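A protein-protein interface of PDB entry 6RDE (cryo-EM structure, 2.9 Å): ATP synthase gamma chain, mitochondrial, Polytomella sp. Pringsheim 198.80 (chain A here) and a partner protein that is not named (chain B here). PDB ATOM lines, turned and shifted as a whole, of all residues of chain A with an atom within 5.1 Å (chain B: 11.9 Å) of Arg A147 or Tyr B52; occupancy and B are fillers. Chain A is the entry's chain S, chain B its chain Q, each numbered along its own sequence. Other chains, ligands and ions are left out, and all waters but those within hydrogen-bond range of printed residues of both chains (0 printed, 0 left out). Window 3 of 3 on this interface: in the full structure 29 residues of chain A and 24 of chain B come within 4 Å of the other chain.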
ATOM      1  N   SER A 141      -9.118  13.722 -13.169  1.00  0.00           N
ATOM      2  CA  SER A 141     -10.370  13.053 -12.866  1.00  0.00           C
ATOM      3  C   SER A 141     -10.458  12.795 -11.376  1.00  0.00           C
ATOM      4  O   SER A 141      -9.474  12.402 -10.746  1.00  0.00           O
ATOM      5  CB  SER A 141     -10.498  11.732 -13.598  1.00  0.00           C
ATOM      6  OG  SER A 141      -9.563  10.801 -13.097  1.00  0.00           O
ATOM      7  N   GLY A 143     -12.348  10.366  -8.742  1.00  0.00           N
ATOM      8  CA  GLY A 143     -13.012   9.084  -8.681  1.00  0.00           C
ATOM      9  C   GLY A 143     -12.244   8.031  -9.455  1.00  0.00           C
ATOM     10  O   GLY A 143     -11.594   8.313 -10.470  1.00  0.00           O
ATOM     11  N   ASP A 144     -12.326   6.789  -8.970  1.00  0.00           N
ATOM     12  CA  ASP A 144     -11.613   5.682  -9.603  1.00  0.00           C
ATOM     13  C   ASP A 144     -12.160   5.359 -10.981  1.00  0.00           C
ATOM     14  O   ASP A 144     -11.421   4.863 -11.835  1.00  0.00           O
ATOM     15  CB  ASP A 144     -11.678   4.442  -8.718  1.00  0.00           C
ATOM     16  CG  ASP A 144     -10.578   4.406  -7.695  1.00  0.00           C
ATOM     17  OD1 ASP A 144      -9.463   4.844  -8.029  1.00  0.00           O
ATOM     18  OD2 ASP A 144     -10.822   3.933  -6.569  1.00  0.00           O
ATOM     19  N   LYS A 145     -13.434   5.640 -11.223  1.00  0.00           N
ATOM     20  CA  LYS A 145     -14.052   5.425 -12.520  1.00  0.00           C
ATOM     21  C   LYS A 145     -13.761   6.545 -13.502  1.00  0.00           C
ATOM     22  O   LYS A 145     -14.265   6.508 -14.626  1.00  0.00           O
ATOM     23  CB  LYS A 145     -15.562   5.268 -12.362  1.00  0.00           C
ATOM     24  CG  LYS A 145     -15.972   4.029 -11.605  1.00  0.00           C
ATOM     25  CD  LYS A 145     -15.646   2.769 -12.390  1.00  0.00           C
ATOM     26  CE  LYS A 145     -16.369   2.737 -13.726  1.00  0.00           C
ATOM     27  NZ  LYS A 145     -17.826   3.002 -13.589  1.00  0.00           N
ATOM     28  N   GLY A 146     -12.975   7.539 -13.104  1.00  0.00           N
ATOM     29  CA  GLY A 146     -12.615   8.622 -13.995  1.00  0.00           C
ATOM     30  C   GLY A 146     -11.296   8.374 -14.685  1.00  0.00           C
ATOM     31  O   GLY A 146     -11.188   8.564 -15.896  1.00  0.00           O
ATOM     32  N   ARG A 147     -10.288   7.946 -13.919  1.00  0.00           N
ATOM     33  CA  ARG A 147      -8.996   7.588 -14.493  1.00  0.00           C
ATOM     34  C   ARG A 147      -9.106   6.369 -15.388  1.00  0.00           C
ATOM     35  O   ARG A 147      -8.423   6.281 -16.414  1.00  0.00           O
ATOM     36  CB  ARG A 147      -7.983   7.320 -13.383  1.00  0.00           C
ATOM     37  CG  ARG A 147      -8.508   6.486 -12.228  1.00  0.00           C
ATOM     38  CD  ARG A 147      -7.365   6.065 -11.318  1.00  0.00           C
ATOM     39  NE  ARG A 147      -7.679   4.881 -10.525  1.00  0.00           N
ATOM     40  CZ  ARG A 147      -7.546   3.631 -10.955  1.00  0.00           C
ATOM     41  NH1 ARG A 147      -7.852   2.621 -10.154  1.00  0.00           N
ATOM     42  NH2 ARG A 147      -7.115   3.387 -12.184  1.00  0.00           N
ATOM     43  N   SER A 148      -9.994   5.447 -15.039  1.00  0.00           N
ATOM     44  CA  SER A 148     -10.167   4.210 -15.774  1.00  0.00           C
ATOM     45  C   SER A 148     -10.947   4.395 -17.065  1.00  0.00           C
ATOM     46  O   SER A 148     -11.110   3.427 -17.815  1.00  0.00           O
ATOM     47  CB  SER A 148     -10.860   3.198 -14.871  1.00  0.00           C
ATOM     48  OG  SER A 148     -10.026   2.848 -13.780  1.00  0.00           O
ATOM     49  N   GLN A 149     -11.436   5.605 -17.329  1.00  0.00           N
ATOM     50  CA  GLN A 149     -12.095   5.935 -18.578  1.00  0.00           C
ATOM     51  C   GLN A 149     -11.580   7.213 -19.214  1.00  0.00           C
ATOM     52  O   GLN A 149     -12.147   7.644 -20.223  1.00  0.00           O
ATOM     53  CB  GLN A 149     -13.607   6.067 -18.370  1.00  0.00           C
ATOM     54  CG  GLN A 149     -14.321   4.750 -18.284  1.00  0.00           C
ATOM     55  CD  GLN A 149     -15.674   4.887 -17.640  1.00  0.00           C
ATOM     56  OE1 GLN A 149     -16.320   5.924 -17.763  1.00  0.00           O
ATOM     57  NE2 GLN A 149     -16.106   3.848 -16.934  1.00  0.00           N
ATOM     58  N   LEU A 150     -10.556   7.848 -18.654  1.00  0.00           N
ATOM     59  CA  LEU A 150      -9.958   9.001 -19.311  1.00  0.00           C
ATOM     60  C   LEU A 150      -8.640   8.669 -19.984  1.00  0.00           C
ATOM     61  O   LEU A 150      -8.302   9.294 -20.991  1.00  0.00           O
ATOM     62  CB  LEU A 150      -9.754  10.147 -18.323  1.00  0.00           C
ATOM     63  CG  LEU A 150     -10.983  11.047 -18.246  1.00  0.00           C
ATOM     64  CD1 LEU A 150     -10.783  12.127 -17.223  1.00  0.00           C
ATOM     65  CD2 LEU A 150     -11.292  11.647 -19.613  1.00  0.00           C
ATOM     66  N   THR A 151      -7.895   7.687 -19.476  1.00  0.00           N
ATOM     67  CA  THR A 151      -6.749   7.190 -20.226  1.00  0.00           C
ATOM     68  C   THR A 151      -7.167   6.406 -21.462  1.00  0.00           C
ATOM     69  O   THR A 151      -6.325   6.161 -22.334  1.00  0.00           O
ATOM     70  CB  THR A 151      -5.859   6.318 -19.335  1.00  0.00           C
ATOM     71  OG1 THR A 151      -6.524   5.083 -19.046  1.00  0.00           O
ATOM     72  CG2 THR A 151      -5.535   7.029 -18.030  1.00  0.00           C
ATOM     73  N   TYR A 158      -3.679  13.529 -19.481  1.00  0.00           N
ATOM     74  CA  TYR A 158      -4.072  13.112 -18.149  1.00  0.00           C
ATOM     75  C   TYR A 158      -2.851  13.141 -17.241  1.00  0.00           C
ATOM     76  O   TYR A 158      -1.842  12.492 -17.533  1.00  0.00           O
ATOM     77  CB  TYR A 158      -4.676  11.716 -18.186  1.00  0.00           C
ATOM     78  CG  TYR A 158      -5.384  11.377 -16.917  1.00  0.00           C
ATOM     79  CD1 TYR A 158      -4.779  10.587 -15.952  1.00  0.00           C
ATOM     80  CD2 TYR A 158      -6.649  11.868 -16.669  1.00  0.00           C
ATOM     81  CE1 TYR A 158      -5.430  10.286 -14.785  1.00  0.00           C
ATOM     82  CE2 TYR A 158      -7.302  11.574 -15.515  1.00  0.00           C
ATOM     83  CZ  TYR A 158      -6.691  10.786 -14.580  1.00  0.00           C
ATOM     84  OH  TYR A 158      -7.357  10.506 -13.424  1.00  0.00           O
ATOM     85  N   GLN A 159      -2.938  13.896 -16.148  1.00  0.00           N
ATOM     86  CA  GLN A 159      -1.758  14.106 -15.320  1.00  0.00           C
ATOM     87  C   GLN A 159      -1.985  13.779 -13.849  1.00  0.00           C
ATOM     88  O   GLN A 159      -1.026  13.506 -13.121  1.00  0.00           O
ATOM     89  CB  GLN A 159      -1.256  15.544 -15.458  1.00  0.00           C
ATOM     90  CG  GLN A 159      -0.697  15.876 -16.829  1.00  0.00           C
ATOM     91  CD  GLN A 159       0.520  16.778 -16.765  1.00  0.00           C
ATOM     92  OE1 GLN A 159       0.462  17.884 -16.237  1.00  0.00           O
ATOM     93  NE2 GLN A 159       1.629  16.308 -17.314  1.00  0.00           N
ATOM     94  N   LEU A 160      -3.231  13.814 -13.391  1.00  0.00           N
ATOM     95  CA  LEU A 160      -3.504  13.677 -11.969  1.00  0.00           C
ATOM     96  C   LEU A 160      -4.791  12.901 -11.754  1.00  0.00           C
ATOM     97  O   LEU A 160      -5.760  13.069 -12.495  1.00  0.00           O
ATOM     98  CB  LEU A 160      -3.582  15.054 -11.308  1.00  0.00           C
ATOM     99  CG  LEU A 160      -3.996  15.221  -9.853  1.00  0.00           C
ATOM    100  CD1 LEU A 160      -2.963  14.666  -8.901  1.00  0.00           C
ATOM    101  CD2 LEU A 160      -4.215  16.684  -9.607  1.00  0.00           C
ATOM    102  N   ALA A 161      -4.787  12.045 -10.734  1.00  0.00           N
ATOM    103  CA  ALA A 161      -5.938  11.219 -10.397  1.00  0.00           C
ATOM    104  C   ALA A 161      -6.224  11.362  -8.914  1.00  0.00           C
ATOM    105  O   ALA A 161      -5.405  10.955  -8.086  1.00  0.00           O
ATOM    106  CB  ALA A 161      -5.686   9.751 -10.739  1.00  0.00           C
ATOM    107  N   PHE B  47      -8.654  11.628   1.255  1.00  0.00           N
ATOM    108  CA  PHE B  47      -8.618  11.319  -0.166  1.00  0.00           C
ATOM    109  C   PHE B  47      -7.191  10.936  -0.519  1.00  0.00           C
ATOM    110  O   PHE B  47      -6.299  10.938   0.331  1.00  0.00           O
ATOM    111  CB  PHE B  47      -9.131  12.483  -1.019  1.00  0.00           C
ATOM    112  CG  PHE B  47      -8.188  13.642  -1.127  1.00  0.00           C
ATOM    113  CD1 PHE B  47      -7.988  14.495  -0.060  1.00  0.00           C
ATOM    114  CD2 PHE B  47      -7.534  13.901  -2.316  1.00  0.00           C
ATOM    115  CE1 PHE B  47      -7.135  15.559  -0.172  1.00  0.00           C
ATOM    116  CE2 PHE B  47      -6.684  14.968  -2.437  1.00  0.00           C
ATOM    117  CZ  PHE B  47      -6.481  15.793  -1.367  1.00  0.00           C
ATOM    118  N   ARG B  48      -6.979  10.596  -1.780  1.00  0.00           N
ATOM    119  CA  ARG B  48      -5.650  10.266  -2.254  1.00  0.00           C
ATOM    120  C   ARG B  48      -5.466  10.838  -3.645  1.00  0.00           C
ATOM    121  O   ARG B  48      -6.361  10.775  -4.490  1.00  0.00           O
ATOM    122  CB  ARG B  48      -5.395   8.746  -2.241  1.00  0.00           C
ATOM    123  CG  ARG B  48      -6.355   7.902  -3.076  1.00  0.00           C
ATOM    124  CD  ARG B  48      -5.950   6.444  -3.136  1.00  0.00           C
ATOM    125  NE  ARG B  48      -6.939   5.639  -3.844  1.00  0.00           N
ATOM    126  CZ  ARG B  48      -6.979   5.479  -5.164  1.00  0.00           C
ATOM    127  NH1 ARG B  48      -7.916   4.720  -5.707  1.00  0.00           N
ATOM    128  NH2 ARG B  48      -6.091   6.081  -5.944  1.00  0.00           N
ATOM    129  N   GLN B  49      -4.306  11.436  -3.867  1.00  0.00           N
ATOM    130  CA  GLN B  49      -3.973  11.977  -5.171  1.00  0.00           C
ATOM    131  C   GLN B  49      -2.781  11.217  -5.715  1.00  0.00           C
ATOM    132  O   GLN B  49      -1.972  10.666  -4.969  1.00  0.00           O
ATOM    133  CB  GLN B  49      -3.675  13.476  -5.115  1.00  0.00           C
ATOM    134  CG  GLN B  49      -2.610  13.855  -4.117  1.00  0.00           C
ATOM    135  CD  GLN B  49      -2.308  15.330  -4.125  1.00  0.00           C
ATOM    136  OE1 GLN B  49      -2.770  16.066  -4.994  1.00  0.00           O
ATOM    137  NE2 GLN B  49      -1.532  15.776  -3.150  1.00  0.00           N
ATOM    138  N   ALA B  50      -2.692  11.187  -7.038  1.00  0.00           N
ATOM    139  CA  ALA B  50      -1.669  10.445  -7.687  1.00  0.00           C
ATOM    140  C   ALA B  50      -1.284  11.209  -8.942  1.00  0.00           C
ATOM    141  O   ALA B  50      -2.160  11.473  -9.779  1.00  0.00           O
ATOM    142  CB  ALA B  50      -2.138   9.037  -8.047  1.00  0.00           C
ATOM    143  N   PRO B  51      -0.024  11.611  -9.083  1.00  0.00           N
ATOM    144  CA  PRO B  51       0.428  12.154 -10.366  1.00  0.00           C
ATOM    145  C   PRO B  51       0.495  11.052 -11.404  1.00  0.00           C
ATOM    146  O   PRO B  51       0.912   9.931 -11.111  1.00  0.00           O
ATOM    147  CB  PRO B  51       1.819  12.710 -10.048  1.00  0.00           C
ATOM    148  CG  PRO B  51       1.833  12.876  -8.569  1.00  0.00           C
ATOM    149  CD  PRO B  51       0.991  11.776  -8.032  1.00  0.00           C
ATOM    150  N   TYR B  52       0.067  11.369 -12.621  1.00  0.00           N
ATOM    151  CA  TYR B  52       0.036  10.403 -13.713  1.00  0.00           C
ATOM    152  C   TYR B  52       0.885  10.939 -14.857  1.00  0.00           C
ATOM    153  O   TYR B  52       0.410  11.736 -15.668  1.00  0.00           O
ATOM    154  CB  TYR B  52      -1.394  10.144 -14.169  1.00  0.00           C
ATOM    155  CG  TYR B  52      -1.997   8.892 -13.589  1.00  0.00           C
ATOM    156  CD1 TYR B  52      -2.256   7.792 -14.394  1.00  0.00           C
ATOM    157  CD2 TYR B  52      -2.304   8.805 -12.240  1.00  0.00           C
ATOM    158  CE1 TYR B  52      -2.805   6.641 -13.877  1.00  0.00           C
ATOM    159  CE2 TYR B  52      -2.855   7.658 -11.710  1.00  0.00           C
ATOM    160  CZ  TYR B  52      -3.104   6.578 -12.537  1.00  0.00           C
ATOM    161  OH  TYR B  52      -3.657   5.428 -12.020  1.00  0.00           O
ATOM    162  N   VAL B  53       2.124  10.472 -14.951  1.00  0.00           N
ATOM    163  CA  VAL B  53       3.063  11.080 -15.883  1.00  0.00           C
ATOM    164  C   VAL B  53       2.954  10.513 -17.296  1.00  0.00           C
ATOM    165  O   VAL B  53       3.095  11.258 -18.271  1.00  0.00           O
ATOM    166  CB  VAL B  53       4.494  10.942 -15.339  1.00  0.00           C
ATOM    167  CG1 VAL B  53       4.735  11.953 -14.230  1.00  0.00           C
ATOM    168  CG2 VAL B  53       4.728   9.528 -14.803  1.00  0.00           C
ATOM    169  N   ASP B  54       2.693   9.215 -17.438  1.00  0.00           N
ATOM    170  CA  ASP B  54       2.814   8.556 -18.729  1.00  0.00           C
ATOM    171  C   ASP B  54       1.487   8.121 -19.330  1.00  0.00           C
ATOM    172  O   ASP B  54       1.450   7.774 -20.513  1.00  0.00           O
ATOM    173  CB  ASP B  54       3.750   7.343 -18.616  1.00  0.00           C
ATOM    174  CG  ASP B  54       3.195   6.247 -17.724  1.00  0.00           C
ATOM    175  OD1 ASP B  54       2.416   6.553 -16.795  1.00  0.00           O
ATOM    176  OD2 ASP B  54       3.567   5.076 -17.942  1.00  0.00           O
ATOM    177  N   GLY B  55       0.412   8.126 -18.556  1.00  0.00           N
ATOM    178  CA  GLY B  55      -0.856   7.643 -19.054  1.00  0.00           C
ATOM    179  C   GLY B  55      -1.173   6.347 -18.353  1.00  0.00           C
ATOM    180  O   GLY B  55      -2.281   5.813 -18.451  1.00  0.00           O
ATOM    181  N   LYS B  56      -0.173   5.835 -17.640  1.00  0.00           N
ATOM    182  CA  LYS B  56      -0.246   4.523 -17.024  1.00  0.00           C
ATOM    183  C   LYS B  56       0.085   4.508 -15.541  1.00  0.00           C
ATOM    184  O   LYS B  56      -0.616   3.820 -14.790  1.00  0.00           O
ATOM    185  CB  LYS B  56       0.703   3.554 -17.756  1.00  0.00           C
ATOM    186  CG  LYS B  56       0.741   2.117 -17.254  1.00  0.00           C
ATOM    187  CD  LYS B  56       1.719   1.286 -18.082  1.00  0.00           C
ATOM    188  CE  LYS B  56       1.807  -0.148 -17.578  1.00  0.00           C
ATOM    189  NZ  LYS B  56       2.758  -0.987 -18.350  1.00  0.00           N
ATOM    190  N   ALA B  57       1.080   5.255 -15.083  1.00  0.00           N
ATOM    191  CA  ALA B  57       1.605   5.039 -13.743  1.00  0.00           C
ATOM    192  C   ALA B  57       1.920   6.344 -13.019  1.00  0.00           C
ATOM    193  O   ALA B  57       1.750   7.443 -13.546  1.00  0.00           O
ATOM    194  CB  ALA B  57       2.859   4.162 -13.802  1.00  0.00           C
ATOM    195  N   GLY B  58       2.377   6.189 -11.781  1.00  0.00           N
ATOM    196  CA  GLY B  58       2.832   7.296 -10.963  1.00  0.00           C
ATOM    197  C   GLY B  58       2.774   6.905  -9.504  1.00  0.00           C
ATOM    198  O   GLY B  58       2.270   5.840  -9.140  1.00  0.00           O
ATOM    199  N   ALA B  59       3.288   7.796  -8.663  1.00  0.00           N
ATOM    200  CA  ALA B  59       3.247   7.609  -7.218  1.00  0.00           C
ATOM    201  C   ALA B  59       1.877   8.049  -6.708  1.00  0.00           C
ATOM    202  O   ALA B  59       1.051   8.550  -7.467  1.00  0.00           O
ATOM    203  CB  ALA B  59       4.383   8.378  -6.541  1.00  0.00           C
ATOM    204  N   SER B  60       1.625   7.862  -5.413  1.00  0.00           N
ATOM    205  CA  SER B  60       0.350   8.274  -4.840  1.00  0.00           C
ATOM    206  C   SER B  60       0.570   8.797  -3.427  1.00  0.00           C
ATOM    207  O   SER B  60       1.504   8.393  -2.728  1.00  0.00           O
ATOM    208  CB  SER B  60      -0.673   7.129  -4.862  1.00  0.00           C
ATOM    209  OG  SER B  60      -0.309   6.075  -3.990  1.00  0.00           O
ATOM    210  N   LYS B  61      -0.329   9.684  -2.998  1.00  0.00           N
ATOM    211  CA  LYS B  61      -0.166  10.423  -1.754  1.00  0.00           C
ATOM    212  C   LYS B  61      -1.485  10.498  -1.004  1.00  0.00           C
ATOM    213  O   LYS B  61      -2.375  11.269  -1.367  1.00  0.00           O
ATOM    214  CB  LYS B  61       0.365  11.831  -2.027  1.00  0.00           C
ATOM    215  CG  LYS B  61       1.009  12.491  -0.815  1.00  0.00           C
ATOM    216  CD  LYS B  61       0.878  14.002  -0.854  1.00  0.00           C
ATOM    217  CE  LYS B  61       1.548  14.581  -2.091  1.00  0.00           C
ATOM    218  NZ  LYS B  61       1.591  16.071  -2.072  1.00  0.00           N
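O of Ala B50 is in hydrogen-bond range of N of Ala A161.
O of Tyr B52 lies close to O of Tyr A158 (3.0 Å).
N of Tyr B52 lies within hydrogen-bond range of O of Gln A159, at 2.5 Å.
The guanidinium group (NH1) of Arg B48 lies within salt-bridge range of the side-chain carboxylate (OD1) of Asp A144, at 2.8 Å.
The backbone carbonyl oxygen (O) of Arg A147 sits close to the side-chain hydroxyl (OG1) of Thr A151, 3.5 Å away.
The backbone NH (N) of Lys B61 lies within hydrogen-bond range of the backbone carbonyl oxygen (O) of Gln B49.
The side-chain hydroxyl (OG) of Ser A141 is in hydrogen-bond range of the backbone NH (N) of Arg A147, 3.1 Å away.
The guanidinium group (NE) of Arg A147 is in salt-bridge range of the side-chain carboxylate (OD1) of Asp A144 (3.1 Å).
The side-chain hydroxyl (OG) of Ser A148 sits at hydrogen-bond distance from the backbone carbonyl oxygen (O) of Asp A144 (3.1 Å).
The backbone NH (N) of Ser A141 sits at hydrogen-bond distance from the backbone carbonyl oxygen (O) of Leu A160, 3.5 Å away.
Arg A147 touches Tyr B52 (CD to OH, 3.8 Å).
Gly B55 touches Thr A151 (O to CG2, 3.5 Å).
Gln A159 touches Pro B51.
CA of Leu A160 touches O of Ala B50, 3.4 Å away.
Ala A161 touches Arg B48 (O to O, 3.7 Å).
Ala A161 touches Gln B49 (O to CA, 3.4 Å).
CE2 of Tyr B52 touches CB of Ala A161, 3.7 Å away.
Printed residues of chain B within 4 Å of Arg A147: Tyr B52 (3.8 Å).
Tyr B52 touches just these residues of chain A: Arg A147, Tyr A158, Gln A159 and Ala A161.
No residue of chain B comes within 4 Å of Ser A141.
No residue of chain B comes within 4 Å of Gly A143.
No residue of chain B comes within 4 Å of Gly A146.
Ser A148 touches none of the printed residues of chain B.
No residue of chain B comes within 4 Å of Gln A149.
Of the printed residues of chain B, Thr A151 touches Gly B55 (3.5 Å).
Of the printed residues of chain B, Tyr A158 touches Tyr B52 (3.0 Å).
Leu A160 touches one residue of chain B.
Ala A161 touches just these residues of chain B: Arg B48, Gln B49, Ala B50 and Tyr B52.
Printed residues of chain A within 4 Å of Gly B55: Thr A151.
Of the printed residues of chain A, Ala B50 touches Leu A160 (3.4 Å) and Ala A161 (2.9 Å).
Of the printed residues of chain A, Pro B51 touches Gln A159.
Of the printed residues of chain A, Gln B49 touches Ala A161.
Of the printed residues of chain A, Arg B48 touches Asp A144 (2.8 Å) and Ala A161 (3.7 Å).
The nearest residue of chain B that does not touch Arg A147 is Arg B48 (4.8 Å).
The nearest printed residue of chain A that does not touch Pro B51 is Leu A160 (4.2 Å).
Of the 14 printed residues of chain A, 7 touch a printed residue of chain B.
Hydrophobic or aromatic side chains of chain A within 4 Å of the printed part of chain B: Tyr A158, Leu A160 and Ala A161.
Of the 15 printed residues of chain B, 6 touch a printed residue of chain A.
Along chain B the printed residues that touch a printed residue of chain A span positions 48 to 55.
Among the printed residues, 11 pairs touch across the chains.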
